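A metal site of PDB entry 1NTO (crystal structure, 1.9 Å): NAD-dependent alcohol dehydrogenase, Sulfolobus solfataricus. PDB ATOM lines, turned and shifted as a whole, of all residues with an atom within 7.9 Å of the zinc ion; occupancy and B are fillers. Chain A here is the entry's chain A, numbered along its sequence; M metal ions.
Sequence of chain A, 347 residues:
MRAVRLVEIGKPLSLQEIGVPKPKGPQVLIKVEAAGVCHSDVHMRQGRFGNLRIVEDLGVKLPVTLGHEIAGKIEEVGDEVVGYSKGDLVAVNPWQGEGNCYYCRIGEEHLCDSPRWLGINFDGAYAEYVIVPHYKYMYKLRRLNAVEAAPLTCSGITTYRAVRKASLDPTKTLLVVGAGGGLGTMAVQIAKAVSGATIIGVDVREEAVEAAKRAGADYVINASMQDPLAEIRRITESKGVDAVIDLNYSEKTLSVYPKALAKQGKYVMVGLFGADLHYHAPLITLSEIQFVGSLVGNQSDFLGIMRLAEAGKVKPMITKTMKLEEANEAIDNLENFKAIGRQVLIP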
ATOM      1  N   GLY A  36     -30.162  23.615 -26.535  1.00  0.00           N
ATOM      2  CA  GLY A  36     -29.758  24.706 -25.678  1.00  0.00           C
ATOM      3  C   GLY A  36     -30.146  26.061 -26.263  1.00  0.00           C
ATOM      4  O   GLY A  36     -30.200  26.227 -27.475  1.00  0.00           O
ATOM      5  N   VAL A  37     -30.441  27.008 -25.382  1.00  0.00           N
ATOM      6  CA  VAL A  37     -30.788  28.380 -25.766  1.00  0.00           C
ATOM      7  C   VAL A  37     -29.710  29.276 -25.162  1.00  0.00           C
ATOM      8  O   VAL A  37     -29.414  29.163 -23.983  1.00  0.00           O
ATOM      9  CB  VAL A  37     -32.192  28.806 -25.195  1.00  0.00           C
ATOM     10  CG1 VAL A  37     -32.488  30.264 -25.547  1.00  0.00           C
ATOM     11  CG2 VAL A  37     -33.303  27.894 -25.740  1.00  0.00           C
ATOM     12  N   CYS A  38     -29.115  30.156 -25.954  1.00  0.00           N
ATOM     13  CA  CYS A  38     -28.116  31.063 -25.383  1.00  0.00           C
ATOM     14  C   CYS A  38     -28.296  32.510 -25.855  1.00  0.00           C
ATOM     15  O   CYS A  38     -29.102  32.795 -26.735  1.00  0.00           O
ATOM     16  CB  CYS A  38     -26.696  30.584 -25.674  1.00  0.00           C
ATOM     17  SG  CYS A  38     -26.049  31.065 -27.307  1.00  0.00           S
ATOM     18  N   HIS A  39     -27.534  33.413 -25.251  1.00  0.00           N
ATOM     19  CA  HIS A  39     -27.664  34.839 -25.545  1.00  0.00           C
ATOM     20  C   HIS A  39     -27.688  35.086 -27.048  1.00  0.00           C
ATOM     21  O   HIS A  39     -28.379  35.985 -27.521  1.00  0.00           O
ATOM     22  CB  HIS A  39     -26.518  35.630 -24.928  1.00  0.00           C
ATOM     23  CG  HIS A  39     -26.735  37.116 -24.947  1.00  0.00           C
ATOM     24  ND1 HIS A  39     -27.553  37.787 -24.061  1.00  0.00           N
ATOM     25  CD2 HIS A  39     -26.286  38.053 -25.811  1.00  0.00           C
ATOM     26  CE1 HIS A  39     -27.565  39.086 -24.409  1.00  0.00           C
ATOM     27  NE2 HIS A  39     -26.812  39.299 -25.476  1.00  0.00           N
ATOM     28  N   SER A  40     -26.917  34.287 -27.791  1.00  0.00           N
ATOM     29  CA  SER A  40     -26.841  34.452 -29.237  1.00  0.00           C
ATOM     30  C   SER A  40     -28.220  34.480 -29.869  1.00  0.00           C
ATOM     31  O   SER A  40     -28.468  35.221 -30.819  1.00  0.00           O
ATOM     32  CB  SER A  40     -26.048  33.305 -29.876  1.00  0.00           C
ATOM     33  OG  SER A  40     -24.747  33.218 -29.322  1.00  0.00           O
ATOM     34  N   ASP A  41     -29.128  33.658 -29.347  1.00  0.00           N
ATOM     35  CA  ASP A  41     -30.462  33.600 -29.910  1.00  0.00           C
ATOM     36  C   ASP A  41     -31.242  34.890 -29.646  1.00  0.00           C
ATOM     37  O   ASP A  41     -32.179  35.204 -30.371  1.00  0.00           O
ATOM     38  CB  ASP A  41     -31.213  32.382 -29.355  1.00  0.00           C
ATOM     39  CG  ASP A  41     -30.608  31.068 -29.833  1.00  0.00           C
ATOM     40  OD1 ASP A  41     -30.225  30.979 -31.009  1.00  0.00           O
ATOM     41  OD2 ASP A  41     -30.539  30.111 -29.031  1.00  0.00           O
ATOM     42  N   PHE A  49     -26.176  38.510 -35.945  1.00  0.00           N
ATOM     43  CA  PHE A  49     -25.254  37.618 -35.240  1.00  0.00           C
ATOM     44  C   PHE A  49     -23.997  38.432 -34.960  1.00  0.00           C
ATOM     45  O   PHE A  49     -23.038  38.390 -35.722  1.00  0.00           O
ATOM     46  CB  PHE A  49     -24.906  36.407 -36.123  1.00  0.00           C
ATOM     47  CG  PHE A  49     -24.107  35.343 -35.396  1.00  0.00           C
ATOM     48  CD1 PHE A  49     -24.733  34.456 -34.538  1.00  0.00           C
ATOM     49  CD2 PHE A  49     -22.722  35.277 -35.542  1.00  0.00           C
ATOM     50  CE1 PHE A  49     -24.001  33.493 -33.835  1.00  0.00           C
ATOM     51  CE2 PHE A  49     -21.986  34.322 -34.834  1.00  0.00           C
ATOM     52  CZ  PHE A  49     -22.623  33.432 -33.985  1.00  0.00           C
ATOM     53  N   GLY A  67     -31.710  27.248 -32.989  1.00  0.00           N
ATOM     54  CA  GLY A  67     -31.198  26.170 -32.151  1.00  0.00           C
ATOM     55  C   GLY A  67     -29.864  25.633 -32.651  1.00  0.00           C
ATOM     56  O   GLY A  67     -29.834  24.765 -33.519  1.00  0.00           O
ATOM     57  N   HIS A  68     -28.767  26.128 -32.106  1.00  0.00           N
ATOM     58  CA  HIS A  68     -27.461  25.672 -32.602  1.00  0.00           C
ATOM     59  C   HIS A  68     -26.737  24.816 -31.565  1.00  0.00           C
ATOM     60  O   HIS A  68     -25.576  24.484 -31.759  1.00  0.00           O
ATOM     61  CB  HIS A  68     -26.592  26.874 -32.984  1.00  0.00           C
ATOM     62  CG  HIS A  68     -26.413  27.846 -31.869  1.00  0.00           C
ATOM     63  ND1 HIS A  68     -27.270  28.905 -31.630  1.00  0.00           N
ATOM     64  CD2 HIS A  68     -25.496  27.885 -30.876  1.00  0.00           C
ATOM     65  CE1 HIS A  68     -26.860  29.517 -30.519  1.00  0.00           C
ATOM     66  NE2 HIS A  68     -25.777  28.921 -30.024  1.00  0.00           N
ATOM     67  N   GLU A  69     -27.426  24.494 -30.478  1.00  0.00           N
ATOM     68  CA  GLU A  69     -26.847  23.707 -29.379  1.00  0.00           C
ATOM     69  C   GLU A  69     -27.667  22.426 -29.356  1.00  0.00           C
ATOM     70  O   GLU A  69     -28.799  22.382 -28.810  1.00  0.00           O
ATOM     71  CB  GLU A  69     -26.935  24.472 -28.059  1.00  0.00           C
ATOM     72  CG  GLU A  69     -26.309  25.878 -28.117  1.00  0.00           C
ATOM     73  CD  GLU A  69     -26.219  26.556 -26.755  1.00  0.00           C
ATOM     74  OE1 GLU A  69     -26.607  25.953 -25.731  1.00  0.00           O
ATOM     75  OE2 GLU A  69     -25.757  27.711 -26.687  1.00  0.00           O
ATOM     76  N   PRO A  94     -22.086  22.495 -34.565  1.00  0.00           N
ATOM     77  CA  PRO A  94     -22.867  23.285 -35.528  1.00  0.00           C
ATOM     78  C   PRO A  94     -22.076  24.246 -36.411  1.00  0.00           C
ATOM     79  O   PRO A  94     -22.633  24.854 -37.343  1.00  0.00           O
ATOM     80  CB  PRO A  94     -23.833  24.037 -34.615  1.00  0.00           C
ATOM     81  CG  PRO A  94     -22.918  24.373 -33.392  1.00  0.00           C
ATOM     82  CD  PRO A  94     -22.100  23.094 -33.217  1.00  0.00           C
ATOM     83  N   TRP A  95     -20.792  24.393 -36.111  1.00  0.00           N
ATOM     84  CA  TRP A  95     -19.974  25.426 -36.740  1.00  0.00           C
ATOM     85  C   TRP A  95     -19.282  24.838 -37.954  1.00  0.00           C
ATOM     86  O   TRP A  95     -18.064  24.619 -37.972  1.00  0.00           O
ATOM     87  CB  TRP A  95     -18.964  25.960 -35.738  1.00  0.00           C
ATOM     88  CG  TRP A  95     -19.596  26.290 -34.443  1.00  0.00           C
ATOM     89  CD1 TRP A  95     -19.401  25.637 -33.260  1.00  0.00           C
ATOM     90  CD2 TRP A  95     -20.573  27.320 -34.194  1.00  0.00           C
ATOM     91  NE1 TRP A  95     -20.203  26.186 -32.289  1.00  0.00           N
ATOM     92  CE2 TRP A  95     -20.926  27.213 -32.829  1.00  0.00           C
ATOM     93  CE3 TRP A  95     -21.174  28.305 -34.978  1.00  0.00           C
ATOM     94  CZ2 TRP A  95     -21.874  28.076 -32.226  1.00  0.00           C
ATOM     95  CZ3 TRP A  95     -22.135  29.169 -34.371  1.00  0.00           C
ATOM     96  CH2 TRP A  95     -22.459  29.038 -33.022  1.00  0.00           C
ATOM     97  N   ILE A 120     -28.454  28.814 -37.335  1.00  0.00           N
ATOM     98  CA  ILE A 120     -28.162  30.229 -37.560  1.00  0.00           C
ATOM     99  C   ILE A 120     -28.484  30.610 -38.983  1.00  0.00           C
ATOM    100  O   ILE A 120     -29.212  31.571 -39.212  1.00  0.00           O
ATOM    101  CB  ILE A 120     -26.700  30.556 -37.191  1.00  0.00           C
ATOM    102  CG1 ILE A 120     -26.490  30.167 -35.717  1.00  0.00           C
ATOM    103  CG2 ILE A 120     -26.415  32.033 -37.431  1.00  0.00           C
ATOM    104  CD1 ILE A 120     -25.372  30.881 -35.024  1.00  0.00           C
ATOM    105  N   TYR A 126     -34.418  23.660 -32.540  1.00  0.00           N
ATOM    106  CA  TYR A 126     -35.727  24.040 -31.964  1.00  0.00           C
ATOM    107  C   TYR A 126     -36.797  23.295 -32.766  1.00  0.00           C
ATOM    108  O   TYR A 126     -37.658  23.899 -33.404  1.00  0.00           O
ATOM    109  CB  TYR A 126     -35.981  25.552 -32.099  1.00  0.00           C
ATOM    110  CG  TYR A 126     -35.200  26.448 -31.154  1.00  0.00           C
ATOM    111  CD1 TYR A 126     -34.056  25.990 -30.483  1.00  0.00           C
ATOM    112  CD2 TYR A 126     -35.567  27.781 -30.995  1.00  0.00           C
ATOM    113  CE1 TYR A 126     -33.301  26.844 -29.689  1.00  0.00           C
ATOM    114  CE2 TYR A 126     -34.809  28.643 -30.196  1.00  0.00           C
ATOM    115  CZ  TYR A 126     -33.671  28.172 -29.560  1.00  0.00           C
ATOM    116  OH  TYR A 126     -32.903  29.032 -28.818  1.00  0.00           O
ATOM    117  N   ALA A 150     -25.607  19.265 -24.794  1.00  0.00           N
ATOM    118  CA  ALA A 150     -25.968  20.255 -25.800  1.00  0.00           C
ATOM    119  C   ALA A 150     -25.277  21.614 -25.632  1.00  0.00           C
ATOM    120  O   ALA A 150     -24.810  22.203 -26.597  1.00  0.00           O
ATOM    121  CB  ALA A 150     -27.511  20.434 -25.861  1.00  0.00           C
ATOM    122  N   PRO A 151     -25.198  22.139 -24.408  1.00  0.00           N
ATOM    123  CA  PRO A 151     -24.554  23.442 -24.205  1.00  0.00           C
ATOM    124  C   PRO A 151     -23.043  23.425 -24.528  1.00  0.00           C
ATOM    125  O   PRO A 151     -22.444  24.471 -24.838  1.00  0.00           O
ATOM    126  CB  PRO A 151     -24.829  23.725 -22.734  1.00  0.00           C
ATOM    127  CG  PRO A 151     -26.138  22.993 -22.489  1.00  0.00           C
ATOM    128  CD  PRO A 151     -25.852  21.686 -23.175  1.00  0.00           C
ATOM    129  N   THR A 153     -21.677  22.331 -27.035  1.00  0.00           N
ATOM    130  CA  THR A 153     -21.468  22.520 -28.472  1.00  0.00           C
ATOM    131  C   THR A 153     -21.318  24.003 -28.824  1.00  0.00           C
ATOM    132  O   THR A 153     -21.017  24.349 -29.979  1.00  0.00           O
ATOM    133  CB  THR A 153     -22.654  21.966 -29.280  1.00  0.00           C
ATOM    134  OG1 THR A 153     -23.822  22.712 -28.975  1.00  0.00           O
ATOM    135  CG2 THR A 153     -22.905  20.488 -28.941  1.00  0.00           C
ATOM    136  N   CYS A 154     -21.530  24.859 -27.826  1.00  0.00           N
ATOM    137  CA  CYS A 154     -21.476  26.298 -28.006  1.00  0.00           C
ATOM    138  C   CYS A 154     -20.572  26.931 -26.929  1.00  0.00           C
ATOM    139  O   CYS A 154     -19.423  27.283 -27.216  1.00  0.00           O
ATOM    140  CB  CYS A 154     -22.896  26.907 -27.952  1.00  0.00           C
ATOM    141  SG  CYS A 154     -22.837  28.692 -28.245  1.00  0.00           S
ATOM    142  N   SER A 155     -21.061  27.028 -25.692  1.00  0.00           N
ATOM    143  CA  SER A 155     -20.236  27.546 -24.590  1.00  0.00           C
ATOM    144  C   SER A 155     -18.989  26.670 -24.301  1.00  0.00           C
ATOM    145  O   SER A 155     -17.919  27.176 -23.948  1.00  0.00           O
ATOM    146  CB  SER A 155     -21.068  27.637 -23.303  1.00  0.00           C
ATOM    147  OG  SER A 155     -22.258  28.398 -23.503  1.00  0.00           O
ATOM    148  N   THR A 158     -16.469  27.150 -27.260  1.00  0.00           N
ATOM    149  CA  THR A 158     -15.969  28.527 -27.172  1.00  0.00           C
ATOM    150  C   THR A 158     -14.915  28.690 -26.060  1.00  0.00           C
ATOM    151  O   THR A 158     -13.826  29.226 -26.293  1.00  0.00           O
ATOM    152  CB  THR A 158     -17.148  29.515 -26.909  1.00  0.00           C
ATOM    153  OG1 THR A 158     -18.006  29.516 -28.049  1.00  0.00           O
ATOM    154  CG2 THR A 158     -16.634  30.940 -26.599  1.00  0.00           C
ATOM    155  N   VAL A 296     -16.432  30.650 -30.902  1.00  0.00           N
ATOM    156  CA  VAL A 296     -16.737  29.255 -31.136  1.00  0.00           C
ATOM    157  C   VAL A 296     -15.445  28.442 -31.326  1.00  0.00           C
ATOM    158  O   VAL A 296     -14.479  28.675 -30.598  1.00  0.00           O
ATOM    159  CB  VAL A 296     -17.773  29.130 -32.296  1.00  0.00           C
ATOM    160  CG1 VAL A 296     -19.000  29.998 -31.939  1.00  0.00           C
ATOM    161  CG2 VAL A 296     -17.236  29.617 -33.616  1.00  0.00           C
ATOM    162  N   ARG A 342     -28.257  27.900 -17.826  1.00  0.00           N
ATOM    163  CA  ARG A 342     -28.449  27.637 -19.240  1.00  0.00           C
ATOM    164  C   ARG A 342     -29.808  26.986 -19.452  1.00  0.00           C
ATOM    165  O   ARG A 342     -30.135  25.974 -18.821  1.00  0.00           O
ATOM    166  CB  ARG A 342     -27.333  26.723 -19.755  1.00  0.00           C
ATOM    167  CG  ARG A 342     -27.524  26.188 -21.172  1.00  0.00           C
ATOM    168  CD  ARG A 342     -27.660  27.315 -22.200  1.00  0.00           C
ATOM    169  NE  ARG A 342     -26.633  28.334 -22.022  1.00  0.00           N
ATOM    170  CZ  ARG A 342     -25.556  28.457 -22.774  1.00  0.00           C
ATOM    171  NH1 ARG A 342     -25.337  27.629 -23.780  1.00  0.00           N
ATOM    172  NH2 ARG A 342     -24.680  29.423 -22.514  1.00  0.00           N
HETATM  173 ZN    ZN M   1     -25.116  29.055 -28.101  1.00  0.00          ZN
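NH1 of Arg 342 is in salt-bridge range of OE1 of Glu 69.
The backbone carbonyl oxygen of Glu 69 sits at hydrogen-bond distance from the backbone NH of Gly 36, at 2.9 Å.
O of Cys 154 sits at hydrogen-bond distance from OG1 of Thr 158, at 2.8 Å.
OG of Ser 40 lies close to SG of Cys 38 (3.2 Å).
The backbone NH of Cys 38 sits at hydrogen-bond distance from the side-chain carboxylate of Asp 41 (3.4 Å).
Four residues have an atom within 4 Å of the zinc ion: Cys 38, His 68, Glu 69 and Cys 154.
The zinc ion is bound by NE2 of His 68, OE2 of Glu 69, SG of Cys 154 and SG of Cys 38.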
